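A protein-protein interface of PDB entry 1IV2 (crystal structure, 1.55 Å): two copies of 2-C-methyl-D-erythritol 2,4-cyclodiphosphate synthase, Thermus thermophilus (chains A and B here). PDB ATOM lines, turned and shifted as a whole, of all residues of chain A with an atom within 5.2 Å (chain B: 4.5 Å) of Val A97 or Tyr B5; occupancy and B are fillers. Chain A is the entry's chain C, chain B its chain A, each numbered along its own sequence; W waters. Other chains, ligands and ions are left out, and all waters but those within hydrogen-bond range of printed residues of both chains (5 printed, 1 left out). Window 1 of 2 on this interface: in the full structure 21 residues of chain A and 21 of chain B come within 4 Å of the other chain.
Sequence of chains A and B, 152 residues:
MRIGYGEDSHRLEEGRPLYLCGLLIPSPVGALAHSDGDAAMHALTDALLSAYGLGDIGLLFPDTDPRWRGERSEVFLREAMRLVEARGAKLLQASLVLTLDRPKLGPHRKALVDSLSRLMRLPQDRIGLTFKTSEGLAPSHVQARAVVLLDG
The side-chain hydroxyl (OG) of Ser B50 lies within hydrogen-bond range of the side-chain hydroxyl (OG) of Ser A95, 2.5 Å away.
OG of Ser A95 is in hydrogen-bond range of N of Tyr B5 (2.9 Å).
OH of Tyr A5 lies within hydrogen-bond range of OH of Tyr B5 (3.2 Å).
NE of Arg B145 lies close to NH1 of Arg A145 (3.5 Å).
The side-chain carboxylate of Glu B7 lies within salt-bridge range of the guanidinium group of Arg A145 (3.0 Å).
The backbone NH (N) of Lys A132 sits at hydrogen-bond distance from the backbone carbonyl oxygen (O) of Leu A98 (2.8 Å).
N of Val A97 sits at hydrogen-bond distance from O of Arg A145 (2.9 Å).
The guanidinium group of Arg A145 lies close to the side-chain amide nitrogen of Gln A143 (3.1 Å).
The backbone carbonyl oxygen (O) of Gly B6 is in hydrogen-bond range of the backbone NH (N) of Ala B146, at 2.7 Å.
The guanidinium group (NE) of Arg B145 lies within salt-bridge range of the side-chain carboxylate (OE1) of Glu B7 (3.1 Å).
The backbone NH (N) of Val A147 lies within hydrogen-bond range of the backbone carbonyl oxygen (O) of Ser A95, 2.9 Å away.
Among the printed residues, pairs that only touch across the chains: Ser A95 with Gly B4 (3.6 Å), Val A97 with Tyr B5 (3.6 Å), Val A97 with Gly B6 (3.9 Å), Val A97 with Glu B7 (3.8 Å), Lys A132 with Glu B7 (3.4 Å) and Arg A145 with Tyr B5 (3.6 Å).
Val A97 touches just these residues of chain B: Tyr B5, Gly B6 and Glu B7.
Tyr B5 touches four residues of chain A.
Of the printed residues of chain B, Ser A95 touches Gly B4 (3.6 Å), Tyr B5 (2.9 Å) and Ser B50 (2.5 Å).
Of the printed residues of chain A, Ser B50 touches Ser A95.
Of the printed residues of chain A, Gly B4 touches Ser A95.
Of the printed residues of chain B, Lys A132 touches Glu B7 (3.4 Å).
Ala A144 touches none of the printed residues of chain B.
The nearest residue of chain A that does not touch Tyr B5 is Val A147 (4.02 Å).
The nearest printed residue of chain A that does not touch Glu B7 is Thr A99 (4.2 Å).
Printed residues of chain B that touch a printed residue of chain A: Gly B4, Tyr B5, Gly B6, Glu B7, Ser B50 and Arg B145.
Hydrophobic or aromatic side chains of chain B within 4 Å of the printed part of chain A: Tyr B5.
Of the 14 printed residues of chain A, 5 touch a printed residue of chain B.
Hydrophobic or aromatic side chains of chain A that line the printed part of chain B: Tyr A5 and Val A97.
Among the printed residues, 11 pairs touch across the chains.
Tyr A5 touches its own counterpart, Tyr B5.
Arg A145 touches Tyr B5, but with the chains exchanged Tyr A5 does not touch Arg B145 (5.1 Å).
Arg A145 touches its own counterpart, Arg B145.
4 positions are printed for both chains.
Of the 11 pairs that touch across the chains among the printed residues, 2 have their exchanged pair printed and touching as well.
Water W1 lies within hydrogen-bond range of the side-chain hydroxyl of Thr A99 (2.6 Å), the side-chain carboxylate of Glu B7 (2.9 Å), the backbone carbonyl oxygen of Val A97 (3.0 Å) and the guanidinium group of Arg A145 (3.5 Å).
Water W3 lies within hydrogen-bond range of the side-chain hydroxyl of Ser B50 (2.7 Å), the backbone carbonyl oxygen of Leu A96 (2.8 Å), the backbone carbonyl oxygen of Tyr B5 (2.8 Å) and the side-chain hydroxyl of Thr A130 (2.8 Å).
Water W4 bridges the side-chain amino group (NZ) of Lys A132 (2.8 Å) and the backbone carbonyl oxygen (O) of Glu B7 (2.9 Å).
Water W5 lies within hydrogen-bond range of OG1 of Thr A130 and N of Glu B7.
Water W2 lies within hydrogen-bond range of the guanidinium group (NH1) of Arg A145 (3.0 Å) and the guanidinium group (NH2) of Arg B145 (3.2 Å).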
ATOM      1  N   TYR A   5     -14.741   5.748  25.475  1.00  0.00           N
ATOM      2  CA  TYR A   5     -15.759   6.789  25.438  1.00  0.00           C
ATOM      3  C   TYR A   5     -15.204   8.063  26.068  1.00  0.00           C
ATOM      4  O   TYR A   5     -14.546   8.017  27.116  1.00  0.00           O
ATOM      5  CB  TYR A   5     -17.010   6.314  26.180  1.00  0.00           C
ATOM      6  CG  TYR A   5     -18.140   7.315  26.182  1.00  0.00           C
ATOM      7  CD1 TYR A   5     -18.893   7.495  25.027  1.00  0.00           C
ATOM      8  CD2 TYR A   5     -18.456   8.076  27.316  1.00  0.00           C
ATOM      9  CE1 TYR A   5     -19.931   8.394  24.969  1.00  0.00           C
ATOM     10  CE2 TYR A   5     -19.509   8.986  27.256  1.00  0.00           C
ATOM     11  CZ  TYR A   5     -20.235   9.138  26.094  1.00  0.00           C
ATOM     12  OH  TYR A   5     -21.281  10.024  25.993  1.00  0.00           O
ATOM     13  N   SER A  95     -16.572   7.387  16.180  1.00  0.00           N
ATOM     14  CA  SER A  95     -17.936   7.842  15.907  1.00  0.00           C
ATOM     15  C   SER A  95     -18.261   8.889  16.956  1.00  0.00           C
ATOM     16  O   SER A  95     -18.180   8.521  18.130  1.00  0.00           O
ATOM     17  CB  SER A  95     -18.940   6.705  15.974  1.00  0.00           C
ATOM     18  OG  SER A  95     -20.247   7.142  15.661  1.00  0.00           O
ATOM     19  N   LEU A  96     -18.583  10.096  16.529  1.00  0.00           N
ATOM     20  CA  LEU A  96     -18.742  11.166  17.520  1.00  0.00           C
ATOM     21  C   LEU A  96     -19.838  12.128  17.109  1.00  0.00           C
ATOM     22  O   LEU A  96     -20.179  12.211  15.932  1.00  0.00           O
ATOM     23  CB  LEU A  96     -17.416  11.907  17.692  1.00  0.00           C
ATOM     24  CG  LEU A  96     -16.987  12.914  16.637  1.00  0.00           C
ATOM     25  CD1 LEU A  96     -15.972  13.900  17.225  1.00  0.00           C
ATOM     26  CD2 LEU A  96     -16.406  12.224  15.419  1.00  0.00           C
ATOM     27  N   VAL A  97     -20.397  12.845  18.056  1.00  0.00           N
ATOM     28  CA  VAL A  97     -21.539  13.720  17.771  1.00  0.00           C
ATOM     29  C   VAL A  97     -21.149  15.110  18.266  1.00  0.00           C
ATOM     30  O   VAL A  97     -20.672  15.169  19.413  1.00  0.00           O
ATOM     31  CB  VAL A  97     -22.818  13.297  18.501  1.00  0.00           C
ATOM     32  CG1 VAL A  97     -23.958  14.262  18.252  1.00  0.00           C
ATOM     33  CG2 VAL A  97     -23.208  11.885  18.074  1.00  0.00           C
ATOM     34  N   LEU A  98     -21.326  16.114  17.438  1.00  0.00           N
ATOM     35  CA  LEU A  98     -21.043  17.473  17.866  1.00  0.00           C
ATOM     36  C   LEU A  98     -22.384  18.193  18.048  1.00  0.00           C
ATOM     37  O   LEU A  98     -23.217  18.111  17.150  1.00  0.00           O
ATOM     38  CB  LEU A  98     -20.148  18.189  16.858  1.00  0.00           C
ATOM     39  CG  LEU A  98     -18.839  17.476  16.544  1.00  0.00           C
ATOM     40  CD1 LEU A  98     -18.059  18.269  15.513  1.00  0.00           C
ATOM     41  CD2 LEU A  98     -18.045  17.301  17.836  1.00  0.00           C
ATOM     42  N   THR A  99     -22.492  18.830  19.218  1.00  0.00           N
ATOM     43  CA  THR A  99     -23.710  19.551  19.551  1.00  0.00           C
ATOM     44  C   THR A  99     -23.387  21.043  19.690  1.00  0.00           C
ATOM     45  O   THR A  99     -22.528  21.404  20.498  1.00  0.00           O
ATOM     46  CB  THR A  99     -24.350  19.035  20.839  1.00  0.00           C
ATOM     47  OG1 THR A  99     -24.579  17.628  20.712  1.00  0.00           O
ATOM     48  CG2 THR A  99     -25.746  19.600  21.036  1.00  0.00           C
ATOM     49  N   THR A 130     -21.611  13.124  13.121  1.00  0.00           N
ATOM     50  CA  THR A 130     -22.963  13.686  13.001  1.00  0.00           C
ATOM     51  C   THR A 130     -23.107  14.986  13.784  1.00  0.00           C
ATOM     52  O   THR A 130     -22.373  15.219  14.763  1.00  0.00           O
ATOM     53  CB  THR A 130     -24.035  12.657  13.456  1.00  0.00           C
ATOM     54  OG1 THR A 130     -23.772  12.380  14.838  1.00  0.00           O
ATOM     55  CG2 THR A 130     -23.926  11.373  12.664  1.00  0.00           C
ATOM     56  N   PHE A 131     -24.030  15.861  13.383  1.00  0.00           N
ATOM     57  CA  PHE A 131     -24.196  17.166  14.026  1.00  0.00           C
ATOM     58  C   PHE A 131     -25.599  17.358  14.582  1.00  0.00           C
ATOM     59  O   PHE A 131     -26.574  16.970  13.936  1.00  0.00           O
ATOM     60  CB  PHE A 131     -23.972  18.343  13.070  1.00  0.00           C
ATOM     61  CG  PHE A 131     -22.702  18.207  12.239  1.00  0.00           C
ATOM     62  CD1 PHE A 131     -21.467  18.031  12.850  1.00  0.00           C
ATOM     63  CD2 PHE A 131     -22.796  18.256  10.857  1.00  0.00           C
ATOM     64  CE1 PHE A 131     -20.319  17.915  12.085  1.00  0.00           C
ATOM     65  CE2 PHE A 131     -21.643  18.123  10.088  1.00  0.00           C
ATOM     66  CZ  PHE A 131     -20.409  17.937  10.696  1.00  0.00           C
ATOM     67  N   LYS A 132     -25.665  17.961  15.765  1.00  0.00           N
ATOM     68  CA  LYS A 132     -26.932  18.262  16.384  1.00  0.00           C
ATOM     69  C   LYS A 132     -26.972  19.716  16.861  1.00  0.00           C
ATOM     70  O   LYS A 132     -25.934  20.225  17.281  1.00  0.00           O
ATOM     71  CB  LYS A 132     -27.171  17.379  17.615  1.00  0.00           C
ATOM     72  CG  LYS A 132     -27.302  15.888  17.451  1.00  0.00           C
ATOM     73  CD  LYS A 132     -28.270  15.475  16.351  1.00  0.00           C
ATOM     74  CE  LYS A 132     -29.623  16.149  16.466  1.00  0.00           C
ATOM     75  NZ  LYS A 132     -30.633  15.507  15.571  1.00  0.00           N
ATOM     76  N   GLN A 143     -20.548  20.949  22.446  1.00  0.00           N
ATOM     77  CA  GLN A 143     -20.329  19.719  23.174  1.00  0.00           C
ATOM     78  C   GLN A 143     -19.934  18.624  22.197  1.00  0.00           C
ATOM     79  O   GLN A 143     -20.385  18.711  21.045  1.00  0.00           O
ATOM     80  CB  GLN A 143     -21.586  19.273  23.907  1.00  0.00           C
ATOM     81  CG  GLN A 143     -22.186  20.378  24.777  1.00  0.00           C
ATOM     82  CD  GLN A 143     -23.600  20.030  25.192  1.00  0.00           C
ATOM     83  OE1 GLN A 143     -24.608  20.523  24.672  1.00  0.00           O
ATOM     84  NE2 GLN A 143     -23.659  19.136  26.170  1.00  0.00           N
ATOM     85  N   ALA A 144     -19.138  17.682  22.677  1.00  0.00           N
ATOM     86  CA  ALA A 144     -18.712  16.567  21.830  1.00  0.00           C
ATOM     87  C   ALA A 144     -18.691  15.293  22.669  1.00  0.00           C
ATOM     88  O   ALA A 144     -18.272  15.394  23.816  1.00  0.00           O
ATOM     89  CB  ALA A 144     -17.339  16.778  21.204  1.00  0.00           C
ATOM     90  N   ARG A 145     -19.141  14.192  22.089  1.00  0.00           N
ATOM     91  CA  ARG A 145     -19.141  12.883  22.724  1.00  0.00           C
ATOM     92  C   ARG A 145     -18.725  11.878  21.637  1.00  0.00           C
ATOM     93  O   ARG A 145     -19.228  11.919  20.510  1.00  0.00           O
ATOM     94  CB  ARG A 145     -20.476  12.491  23.363  1.00  0.00           C
ATOM     95  CG  ARG A 145     -21.012  13.552  24.328  1.00  0.00           C
ATOM     96  CD  ARG A 145     -22.168  13.085  25.223  1.00  0.00           C
ATOM     97  NE  ARG A 145     -22.495  14.168  26.172  1.00  0.00           N
ATOM     98  CZ  ARG A 145     -23.315  15.168  25.862  1.00  0.00           C
ATOM     99  NH1 ARG A 145     -23.919  15.252  24.680  1.00  0.00           N
ATOM    100  NH2 ARG A 145     -23.538  16.103  26.778  1.00  0.00           N
ATOM    101  N   ALA A 146     -17.799  11.016  22.037  1.00  0.00           N
ATOM    102  CA  ALA A 146     -17.090  10.166  21.086  1.00  0.00           C
ATOM    103  C   ALA A 146     -16.836   8.759  21.602  1.00  0.00           C
ATOM    104  O   ALA A 146     -16.497   8.541  22.779  1.00  0.00           O
ATOM    105  CB  ALA A 146     -15.759  10.859  20.752  1.00  0.00           C
ATOM    106  N   VAL A 147     -17.008   7.785  20.719  1.00  0.00           N
ATOM    107  CA  VAL A 147     -16.630   6.410  20.974  1.00  0.00           C
ATOM    108  C   VAL A 147     -15.533   6.012  19.990  1.00  0.00           C
ATOM    109  O   VAL A 147     -15.649   6.309  18.789  1.00  0.00           O
ATOM    110  CB  VAL A 147     -17.771   5.394  20.800  1.00  0.00           C
ATOM    111  CG1 VAL A 147     -17.243   4.003  21.136  1.00  0.00           C
ATOM    112  CG2 VAL A 147     -18.947   5.747  21.693  1.00  0.00           C
ATOM    113  N   GLY B   4     -21.496   2.631  16.066  1.00  0.00           N
ATOM    114  CA  GLY B   4     -21.909   3.998  15.767  1.00  0.00           C
ATOM    115  C   GLY B   4     -22.543   4.602  17.010  1.00  0.00           C
ATOM    116  O   GLY B   4     -23.154   3.871  17.796  1.00  0.00           O
ATOM    117  N   TYR B   5     -22.387   5.915  17.145  1.00  0.00           N
ATOM    118  CA  TYR B   5     -22.938   6.637  18.291  1.00  0.00           C
ATOM    119  C   TYR B   5     -23.780   7.798  17.793  1.00  0.00           C
ATOM    120  O   TYR B   5     -23.321   8.523  16.899  1.00  0.00           O
ATOM    121  CB  TYR B   5     -21.763   7.102  19.159  1.00  0.00           C
ATOM    122  CG  TYR B   5     -22.194   7.916  20.347  1.00  0.00           C
ATOM    123  CD1 TYR B   5     -22.872   7.269  21.395  1.00  0.00           C
ATOM    124  CD2 TYR B   5     -21.934   9.277  20.434  1.00  0.00           C
ATOM    125  CE1 TYR B   5     -23.266   8.021  22.498  1.00  0.00           C
ATOM    126  CE2 TYR B   5     -22.326  10.038  21.523  1.00  0.00           C
ATOM    127  CZ  TYR B   5     -22.992   9.381  22.535  1.00  0.00           C
ATOM    128  OH  TYR B   5     -23.412  10.069  23.651  1.00  0.00           O
ATOM    129  N   GLY B   6     -24.976   7.989  18.330  1.00  0.00           N
ATOM    130  CA  GLY B   6     -25.843   9.080  17.878  1.00  0.00           C
ATOM    131  C   GLY B   6     -26.610   9.685  19.051  1.00  0.00           C
ATOM    132  O   GLY B   6     -26.832   9.002  20.056  1.00  0.00           O
ATOM    133  N   GLU B   7     -26.994  10.949  18.881  1.00  0.00           N
ATOM    134  CA  GLU B   7     -27.746  11.689  19.877  1.00  0.00           C
ATOM    135  C   GLU B   7     -28.919  12.432  19.227  1.00  0.00           C
ATOM    136  O   GLU B   7     -28.907  12.640  18.030  1.00  0.00           O
ATOM    137  CB  GLU B   7     -26.916  12.779  20.563  1.00  0.00           C
ATOM    138  CG  GLU B   7     -25.666  12.269  21.263  1.00  0.00           C
ATOM    139  CD  GLU B   7     -25.061  13.373  22.120  1.00  0.00           C
ATOM    140  OE1 GLU B   7     -25.819  14.177  22.682  1.00  0.00           O
ATOM    141  OE2 GLU B   7     -23.820  13.350  22.201  1.00  0.00           O
ATOM    142  N   ALA B  47     -26.932   6.976  14.655  1.00  0.00           N
ATOM    143  CA  ALA B  47     -25.895   6.023  15.085  1.00  0.00           C
ATOM    144  C   ALA B  47     -25.593   5.049  13.937  1.00  0.00           C
ATOM    145  O   ALA B  47     -24.434   4.781  13.627  1.00  0.00           O
ATOM    146  CB  ALA B  47     -26.274   5.262  16.342  1.00  0.00           C
ATOM    147  N   SER B  50     -23.787   6.836  11.180  1.00  0.00           N
ATOM    148  CA  SER B  50     -22.437   7.089  11.704  1.00  0.00           C
ATOM    149  C   SER B  50     -21.500   5.890  11.565  1.00  0.00           C
ATOM    150  O   SER B  50     -20.305   6.027  11.263  1.00  0.00           O
ATOM    151  CB  SER B  50     -22.538   7.534  13.180  1.00  0.00           C
ATOM    152  OG  SER B  50     -21.309   8.135  13.576  1.00  0.00           O
ATOM    153  N   ARG B 145     -29.573   9.112  23.553  1.00  0.00           N
ATOM    154  CA  ARG B 145     -28.183   8.864  23.158  1.00  0.00           C
ATOM    155  C   ARG B 145     -28.081   7.374  22.891  1.00  0.00           C
ATOM    156  O   ARG B 145     -28.595   6.573  23.686  1.00  0.00           O
ATOM    157  CB  ARG B 145     -27.212   9.377  24.224  1.00  0.00           C
ATOM    158  CG  ARG B 145     -27.327  10.891  24.440  1.00  0.00           C
ATOM    159  CD  ARG B 145     -26.142  11.430  25.221  1.00  0.00           C
ATOM    160  NE  ARG B 145     -26.345  12.874  25.407  1.00  0.00           N
ATOM    161  CZ  ARG B 145     -27.062  13.408  26.379  1.00  0.00           C
ATOM    162  NH1 ARG B 145     -27.670  12.677  27.304  1.00  0.00           N
ATOM    163  NH2 ARG B 145     -27.158  14.737  26.412  1.00  0.00           N
ATOM    164  N   ALA B 146     -27.483   6.983  21.775  1.00  0.00           N
ATOM    165  CA  ALA B 146     -27.549   5.591  21.378  1.00  0.00           C
ATOM    166  C   ALA B 146     -26.214   5.102  20.848  1.00  0.00           C
ATOM    167  O   ALA B 146     -25.531   5.887  20.193  1.00  0.00           O
ATOM    168  CB  ALA B 146     -28.574   5.408  20.242  1.00  0.00           C
ATOM    169  N   VAL B 147     -25.921   3.837  21.109  1.00  0.00           N
ATOM    170  CA  VAL B 147     -24.774   3.153  20.495  1.00  0.00           C
ATOM    171  C   VAL B 147     -25.303   1.960  19.700  1.00  0.00           C
ATOM    172  O   VAL B 147     -26.227   1.295  20.177  1.00  0.00           O
ATOM    173  CB  VAL B 147     -23.770   2.655  21.543  1.00  0.00           C
ATOM    174  CG1 VAL B 147     -22.576   1.997  20.862  1.00  0.00           C
ATOM    175  CG2 VAL B 147     -23.355   3.814  22.448  1.00  0.00           C
HETATM  176  O   HOH W   1     -22.717  15.989  21.484  1.00  0.00           O
HETATM  177  O   HOH W   2     -26.272  17.145  24.504  1.00  0.00           O
HETATM  178  O   HOH W   3     -21.959  10.235  15.126  1.00  0.00           O
HETATM  179  O   HOH W   4     -30.346  12.688  15.504  1.00  0.00           O
HETATM  180  O   HOH W   5     -26.263  12.266  16.218  1.00  0.00           O
